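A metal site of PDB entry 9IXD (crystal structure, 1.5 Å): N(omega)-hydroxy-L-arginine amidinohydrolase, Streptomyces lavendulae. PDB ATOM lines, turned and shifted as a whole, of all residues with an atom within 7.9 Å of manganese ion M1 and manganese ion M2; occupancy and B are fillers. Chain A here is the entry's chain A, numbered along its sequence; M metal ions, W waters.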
ATOM      1  N   THR A  85      30.192  19.377 -35.722  1.00  0.00           N
ATOM      2  CA  THR A  85      29.693  20.329 -34.735  1.00  0.00           C
ATOM      3  C   THR A  85      28.168  20.259 -34.619  1.00  0.00           C
ATOM      4  O   THR A  85      27.468  19.775 -35.511  1.00  0.00           O
ATOM      5  CB  THR A  85      30.071  21.775 -35.078  1.00  0.00           C
ATOM      6  OG1 THR A  85      29.435  22.162 -36.310  1.00  0.00           O
ATOM      7  CG2 THR A  85      31.568  21.956 -35.192  1.00  0.00           C
ATOM      8  N   CYS A  86      27.663  20.741 -33.471  1.00  0.00           N
ATOM      9  CA  CYS A  86      26.225  20.842 -33.313  1.00  0.00           C
ATOM     10  C   CYS A  86      25.595  21.714 -34.390  1.00  0.00           C
ATOM     11  O   CYS A  86      24.414  21.536 -34.702  1.00  0.00           O
ATOM     12  CB  CYS A  86      25.868  21.415 -31.926  1.00  0.00           C
ATOM     13  SG  CYS A  86      26.125  20.236 -30.564  1.00  0.00           S
ATOM     14  N   SER A  87      26.356  22.676 -34.940  1.00  0.00           N
ATOM     15  CA  SER A  87      25.798  23.618 -35.908  1.00  0.00           C
ATOM     16  C   SER A  87      25.317  22.939 -37.182  1.00  0.00           C
ATOM     17  O   SER A  87      24.472  23.509 -37.869  1.00  0.00           O
ATOM     18  CB  SER A  87      26.824  24.706 -36.238  1.00  0.00           C
ATOM     19  OG  SER A  87      27.096  25.476 -35.094  1.00  0.00           O
ATOM     20  N   TYR A 107      17.713  17.001 -27.070  1.00  0.00           N
ATOM     21  CA  TYR A 107      18.947  17.723 -27.365  1.00  0.00           C
ATOM     22  C   TYR A 107      19.863  17.513 -26.157  1.00  0.00           C
ATOM     23  O   TYR A 107      19.711  18.176 -25.119  1.00  0.00           O
ATOM     24  CB  TYR A 107      18.617  19.186 -27.634  1.00  0.00           C
ATOM     25  CG  TYR A 107      19.694  19.935 -28.362  1.00  0.00           C
ATOM     26  CD1 TYR A 107      20.807  20.418 -27.688  1.00  0.00           C
ATOM     27  CD2 TYR A 107      19.610  20.170 -29.728  1.00  0.00           C
ATOM     28  CE1 TYR A 107      21.817  21.104 -28.352  1.00  0.00           C
ATOM     29  CE2 TYR A 107      20.598  20.855 -30.415  1.00  0.00           C
ATOM     30  CZ  TYR A 107      21.716  21.339 -29.720  1.00  0.00           C
ATOM     31  OH  TYR A 107      22.721  22.014 -30.396  1.00  0.00           O
ATOM     32  N   ILE A 108      20.780  16.557 -26.270  1.00  0.00           N
ATOM     33  CA  ILE A 108      21.569  16.083 -25.142  1.00  0.00           C
ATOM     34  C   ILE A 108      22.897  16.815 -25.174  1.00  0.00           C
ATOM     35  O   ILE A 108      23.687  16.622 -26.104  1.00  0.00           O
ATOM     36  CB  ILE A 108      21.725  14.560 -25.185  1.00  0.00           C
ATOM     37  CG1 ILE A 108      20.335  13.906 -25.312  1.00  0.00           C
ATOM     38  CG2 ILE A 108      22.481  14.046 -23.947  1.00  0.00           C
ATOM     39  CD1 ILE A 108      20.361  12.392 -25.288  1.00  0.00           C
ATOM     40  N   ASP A 109      23.142  17.686 -24.193  1.00  0.00           N
ATOM     41  CA  ASP A 109      24.223  18.661 -24.320  1.00  0.00           C
ATOM     42  C   ASP A 109      24.507  19.219 -22.937  1.00  0.00           C
ATOM     43  O   ASP A 109      23.573  19.427 -22.153  1.00  0.00           O
ATOM     44  CB  ASP A 109      23.765  19.754 -25.298  1.00  0.00           C
ATOM     45  CG  ASP A 109      24.883  20.568 -25.873  1.00  0.00           C
ATOM     46  OD1 ASP A 109      25.814  20.997 -25.142  1.00  0.00           O
ATOM     47  OD2 ASP A 109      24.823  20.803 -27.093  1.00  0.00           O
ATOM     48  N   GLY A 110      25.775  19.460 -22.615  1.00  0.00           N
ATOM     49  CA  GLY A 110      26.072  20.167 -21.383  1.00  0.00           C
ATOM     50  C   GLY A 110      25.640  21.620 -21.399  1.00  0.00           C
ATOM     51  O   GLY A 110      25.487  22.238 -20.336  1.00  0.00           O
ATOM     52  N   HIS A 111      25.403  22.171 -22.591  1.00  0.00           N
ATOM     53  CA  HIS A 111      24.949  23.536 -22.805  1.00  0.00           C
ATOM     54  C   HIS A 111      23.499  23.570 -23.256  1.00  0.00           C
ATOM     55  O   HIS A 111      22.905  22.554 -23.633  1.00  0.00           O
ATOM     56  CB  HIS A 111      25.796  24.221 -23.882  1.00  0.00           C
ATOM     57  CG  HIS A 111      27.264  24.214 -23.597  1.00  0.00           C
ATOM     58  ND1 HIS A 111      28.082  23.204 -24.020  1.00  0.00           N
ATOM     59  CD2 HIS A 111      28.042  25.100 -22.935  1.00  0.00           C
ATOM     60  CE1 HIS A 111      29.325  23.464 -23.639  1.00  0.00           C
ATOM     61  NE2 HIS A 111      29.332  24.611 -22.986  1.00  0.00           N
ATOM     62  N   GLY A 112      22.925  24.776 -23.262  1.00  0.00           N
ATOM     63  CA  GLY A 112      21.596  24.938 -23.819  1.00  0.00           C
ATOM     64  C   GLY A 112      21.540  25.199 -25.322  1.00  0.00           C
ATOM     65  O   GLY A 112      20.493  24.979 -25.961  1.00  0.00           O
ATOM     66  N   ASP A 113      22.654  25.646 -25.905  1.00  0.00           N
ATOM     67  CA  ASP A 113      22.759  25.993 -27.327  1.00  0.00           C
ATOM     68  C   ASP A 113      21.556  26.845 -27.774  1.00  0.00           C
ATOM     69  O   ASP A 113      21.011  26.672 -28.864  1.00  0.00           O
ATOM     70  CB  ASP A 113      22.932  24.741 -28.197  1.00  0.00           C
ATOM     71  CG  ASP A 113      24.322  24.107 -28.035  1.00  0.00           C
ATOM     72  OD1 ASP A 113      25.112  24.611 -27.211  1.00  0.00           O
ATOM     73  OD2 ASP A 113      24.619  23.097 -28.754  1.00  0.00           O
ATOM     74  N   TYR A 124      29.584  32.541 -31.148  1.00  0.00           N
ATOM     75  CA  TYR A 124      29.778  31.203 -31.684  1.00  0.00           C
ATOM     76  C   TYR A 124      28.460  30.597 -32.168  1.00  0.00           C
ATOM     77  O   TYR A 124      27.493  30.471 -31.402  1.00  0.00           O
ATOM     78  CB  TYR A 124      30.432  30.295 -30.633  1.00  0.00           C
ATOM     79  CG  TYR A 124      30.667  28.873 -31.060  1.00  0.00           C
ATOM     80  CD1 TYR A 124      31.202  28.576 -32.309  1.00  0.00           C
ATOM     81  CD2 TYR A 124      30.345  27.820 -30.213  1.00  0.00           C
ATOM     82  CE1 TYR A 124      31.420  27.262 -32.704  1.00  0.00           C
ATOM     83  CE2 TYR A 124      30.539  26.512 -30.603  1.00  0.00           C
ATOM     84  CZ  TYR A 124      31.074  26.229 -31.847  1.00  0.00           C
ATOM     85  OH  TYR A 124      31.251  24.925 -32.224  1.00  0.00           O
ATOM     86  N   GLY A 126      27.717  27.576 -32.776  1.00  0.00           N
ATOM     87  CA  GLY A 126      27.357  26.355 -32.079  1.00  0.00           C
ATOM     88  C   GLY A 126      26.601  26.584 -30.800  1.00  0.00           C
ATOM     89  O   GLY A 126      25.986  25.645 -30.281  1.00  0.00           O
ATOM     90  N   GLY A 127      26.614  27.804 -30.266  1.00  0.00           N
ATOM     91  CA  GLY A 127      25.794  28.103 -29.122  1.00  0.00           C
ATOM     92  C   GLY A 127      24.427  28.643 -29.464  1.00  0.00           C
ATOM     93  O   GLY A 127      23.722  29.073 -28.558  1.00  0.00           O
ATOM     94  N   MET A 128      24.059  28.602 -30.746  1.00  0.00           N
ATOM     95  CA  MET A 128      22.827  29.205 -31.273  1.00  0.00           C
ATOM     96  C   MET A 128      21.976  28.191 -32.023  1.00  0.00           C
ATOM     97  O   MET A 128      21.049  28.570 -32.763  1.00  0.00           O
ATOM     98  CB  MET A 128      23.182  30.385 -32.179  1.00  0.00           C
ATOM     99  CG  MET A 128      24.136  31.388 -31.539  1.00  0.00           C
ATOM    100  SD  MET A 128      24.956  32.536 -32.682  1.00  0.00           S
ATOM    101  CE  MET A 128      23.538  33.451 -33.238  1.00  0.00           C
ATOM    102  N   VAL A 129      22.230  26.892 -31.854  1.00  0.00           N
ATOM    103  CA  VAL A 129      21.679  25.876 -32.746  1.00  0.00           C
ATOM    104  C   VAL A 129      20.221  25.628 -32.454  1.00  0.00           C
ATOM    105  O   VAL A 129      19.382  25.613 -33.360  1.00  0.00           O
ATOM    106  CB  VAL A 129      22.496  24.575 -32.621  1.00  0.00           C
ATOM    107  CG1 VAL A 129      21.855  23.447 -33.461  1.00  0.00           C
ATOM    108  CG2 VAL A 129      23.953  24.813 -33.026  1.00  0.00           C
ATOM    109  N   LEU A 130      19.881  25.360 -31.196  1.00  0.00           N
ATOM    110  CA  LEU A 130      18.512  24.972 -30.884  1.00  0.00           C
ATOM    111  C   LEU A 130      17.584  26.165 -31.015  1.00  0.00           C
ATOM    112  O   LEU A 130      16.456  26.017 -31.478  1.00  0.00           O
ATOM    113  CB  LEU A 130      18.463  24.350 -29.481  1.00  0.00           C
ATOM    114  CG  LEU A 130      17.131  23.782 -28.987  1.00  0.00           C
ATOM    115  CD1 LEU A 130      16.589  22.741 -29.967  1.00  0.00           C
ATOM    116  CD2 LEU A 130      17.267  23.184 -27.591  1.00  0.00           C
ATOM    117  N   SER A 155      21.887  19.405 -19.597  1.00  0.00           N
ATOM    118  CA  SER A 155      22.383  20.777 -19.569  1.00  0.00           C
ATOM    119  C   SER A 155      22.502  21.267 -18.132  1.00  0.00           C
ATOM    120  O   SER A 155      21.679  20.913 -17.270  1.00  0.00           O
ATOM    121  CB  SER A 155      21.424  21.679 -20.353  1.00  0.00           C
ATOM    122  OG  SER A 155      21.135  21.099 -21.615  1.00  0.00           O
ATOM    123  N   HIS A 196      19.764  14.104 -30.481  1.00  0.00           N
ATOM    124  CA  HIS A 196      20.938  14.894 -30.852  1.00  0.00           C
ATOM    125  C   HIS A 196      21.881  14.892 -29.648  1.00  0.00           C
ATOM    126  O   HIS A 196      21.486  15.280 -28.554  1.00  0.00           O
ATOM    127  CB  HIS A 196      20.496  16.319 -31.218  1.00  0.00           C
ATOM    128  CG  HIS A 196      21.616  17.308 -31.317  1.00  0.00           C
ATOM    129  ND1 HIS A 196      22.003  17.855 -32.523  1.00  0.00           N
ATOM    130  CD2 HIS A 196      22.448  17.816 -30.383  1.00  0.00           C
ATOM    131  CE1 HIS A 196      23.029  18.673 -32.324  1.00  0.00           C
ATOM    132  NE2 HIS A 196      23.332  18.652 -31.029  1.00  0.00           N
ATOM    133  N   ILE A 197      23.135  14.445 -29.812  1.00  0.00           N
ATOM    134  CA  ILE A 197      24.074  14.389 -28.697  1.00  0.00           C
ATOM    135  C   ILE A 197      25.332  15.184 -28.986  1.00  0.00           C
ATOM    136  O   ILE A 197      25.975  14.964 -30.024  1.00  0.00           O
ATOM    137  CB  ILE A 197      24.482  12.951 -28.337  1.00  0.00           C
ATOM    138  CG1 ILE A 197      23.261  12.136 -27.955  1.00  0.00           C
ATOM    139  CG2 ILE A 197      25.465  12.953 -27.147  1.00  0.00           C
ATOM    140  CD1 ILE A 197      23.581  10.638 -27.889  1.00  0.00           C
ATOM    141  N   ASP A 198      25.678  16.080 -28.066  1.00  0.00           N
ATOM    142  CA  ASP A 198      26.967  16.760 -28.000  1.00  0.00           C
ATOM    143  C   ASP A 198      27.748  16.119 -26.854  1.00  0.00           C
ATOM    144  O   ASP A 198      27.289  16.145 -25.714  1.00  0.00           O
ATOM    145  CB  ASP A 198      26.680  18.242 -27.719  1.00  0.00           C
ATOM    146  CG  ASP A 198      27.907  19.109 -27.467  1.00  0.00           C
ATOM    147  OD1 ASP A 198      29.029  18.620 -27.217  1.00  0.00           O
ATOM    148  OD2 ASP A 198      27.715  20.355 -27.483  1.00  0.00           O
ATOM    149  N   TRP A 199      28.920  15.522 -27.182  1.00  0.00           N
ATOM    150  CA  TRP A 199      29.646  14.753 -26.176  1.00  0.00           C
ATOM    151  C   TRP A 199      30.138  15.580 -25.001  1.00  0.00           C
ATOM    152  O   TRP A 199      30.502  14.999 -23.979  1.00  0.00           O
ATOM    153  CB  TRP A 199      30.817  13.974 -26.831  1.00  0.00           C
ATOM    154  CG  TRP A 199      30.335  12.992 -27.859  1.00  0.00           C
ATOM    155  CD1 TRP A 199      30.680  12.959 -29.199  1.00  0.00           C
ATOM    156  CD2 TRP A 199      29.418  11.895 -27.669  1.00  0.00           C
ATOM    157  NE1 TRP A 199      30.026  11.948 -29.833  1.00  0.00           N
ATOM    158  CE2 TRP A 199      29.244  11.268 -28.923  1.00  0.00           C
ATOM    159  CE3 TRP A 199      28.723  11.393 -26.564  1.00  0.00           C
ATOM    160  CZ2 TRP A 199      28.411  10.167 -29.114  1.00  0.00           C
ATOM    161  CZ3 TRP A 199      27.873  10.292 -26.756  1.00  0.00           C
ATOM    162  CH2 TRP A 199      27.734   9.700 -28.024  1.00  0.00           C
ATOM    163  N   ASP A 200      30.082  16.919 -25.057  1.00  0.00           N
ATOM    164  CA  ASP A 200      30.444  17.648 -23.850  1.00  0.00           C
ATOM    165  C   ASP A 200      29.400  17.489 -22.729  1.00  0.00           C
ATOM    166  O   ASP A 200      29.636  17.961 -21.626  1.00  0.00           O
ATOM    167  CB  ASP A 200      30.728  19.155 -24.122  1.00  0.00           C
ATOM    168  CG  ASP A 200      29.496  19.972 -24.598  1.00  0.00           C
ATOM    169  OD1 ASP A 200      28.351  19.645 -24.219  1.00  0.00           O
ATOM    170  OD2 ASP A 200      29.693  20.990 -25.333  1.00  0.00           O
ATOM    171  N   VAL A 201      28.297  16.773 -22.970  1.00  0.00           N
ATOM    172  CA  VAL A 201      27.380  16.444 -21.899  1.00  0.00           C
ATOM    173  C   VAL A 201      28.017  15.489 -20.889  1.00  0.00           C
ATOM    174  O   VAL A 201      27.591  15.430 -19.734  1.00  0.00           O
ATOM    175  CB  VAL A 201      26.082  15.853 -22.481  1.00  0.00           C
ATOM    176  CG1 VAL A 201      26.308  14.415 -22.956  1.00  0.00           C
ATOM    177  CG2 VAL A 201      24.930  15.945 -21.460  1.00  0.00           C
ATOM    178  N   ALA A 240      27.640  14.374 -32.240  1.00  0.00           N
ATOM    179  CA  ALA A 240      28.395  15.584 -32.536  1.00  0.00           C
ATOM    180  C   ALA A 240      29.463  15.884 -31.501  1.00  0.00           C
ATOM    181  O   ALA A 240      29.304  15.596 -30.297  1.00  0.00           O
ATOM    182  CB  ALA A 240      27.462  16.817 -32.677  1.00  0.00           C
ATOM    183  N   GLU A 241      30.546  16.505 -31.973  1.00  0.00           N
ATOM    184  CA  GLU A 241      31.540  17.185 -31.146  1.00  0.00           C
ATOM    185  C   GLU A 241      32.404  16.222 -30.329  1.00  0.00           C
ATOM    186  O   GLU A 241      32.633  16.401 -29.135  1.00  0.00           O
ATOM    187  CB  GLU A 241      30.879  18.250 -30.264  1.00  0.00           C
ATOM    188  CG  GLU A 241      29.945  19.190 -31.078  1.00  0.00           C
ATOM    189  CD  GLU A 241      30.067  20.679 -30.749  1.00  0.00           C
ATOM    190  OE1 GLU A 241      30.739  21.042 -29.750  1.00  0.00           O
ATOM    191  OE2 GLU A 241      29.464  21.500 -31.487  1.00  0.00           O
HETATM  192 MN    MN M   1      26.235  21.681 -28.545  1.00  0.00          MN
HETATM  193 MN    MN M   2      27.749  21.631 -25.515  1.00  0.00          MN
HETATM  194  O   HOH W   1      27.677  23.120 -29.699  1.00  0.00           O
HETATM  195  O   HOH W   2      27.244  23.056 -26.959  1.00  0.00           O
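Manganese ion M1 is bound by OD2 of Asp 113, OD2 of Asp 109, OD2 of Asp 198, water W2, water W1 and SG of Cys 86.
Manganese ion M2 is bound by the side-chain carboxylate (OD2) of Asp 200 (2.1 Å), the side-chain carboxylate (OD1) of Asp 109 (2.1 Å), water W2 (2.1 Å), a ring nitrogen (ND1) of His 111 (2.2 Å), the side-chain carboxylate (OD2) of Asp 198 (2.3 Å) and the side-chain carboxylate (OD1) of Asp 200 (2.4 Å).
The backbone NH of Gly 110 sits close to the side-chain carboxylate of Asp 200 (3.0 Å).
The side-chain hydroxyl (OG) of Ser 155 sits at hydrogen-bond distance from the backbone carbonyl oxygen (O) of Asp 109, at 3.0 Å.
OH of Tyr 107 lies close to OD2 of Asp 113, 2.7 Å away.
O of Asp 113 is in hydrogen-bond range of N of Val 129 (3.2 Å).
O of Asp 113 is in hydrogen-bond range of N of Leu 130 (2.9 Å).
The backbone NH (N) of Cys 86 is in hydrogen-bond range of the side-chain carboxylate (OE2) of Glu 241 (2.8 Å).
A ring nitrogen (NE2) of His 196 lies close to the side-chain sulfur (SG) of Cys 86 (3.2 Å).
The side-chain hydroxyl (OH) of Tyr 107 sits close to a ring nitrogen (NE2) of His 196, 3.5 Å away.
Of the 25 residues printed, 4 come within 4 Å of manganese ion M2.
Water W1 lies within hydrogen-bond range of OE2 of Glu 241 (3.0 Å) and O of Gly 126 (3.1 Å).
Tyr 107 touches manganese ion M1.
Of the 25 residues printed, 5 come within 4 Å of manganese ion M1.
The nearest printed residue that does not touch manganese ion M1 is Gly 126 (4.3 Å).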
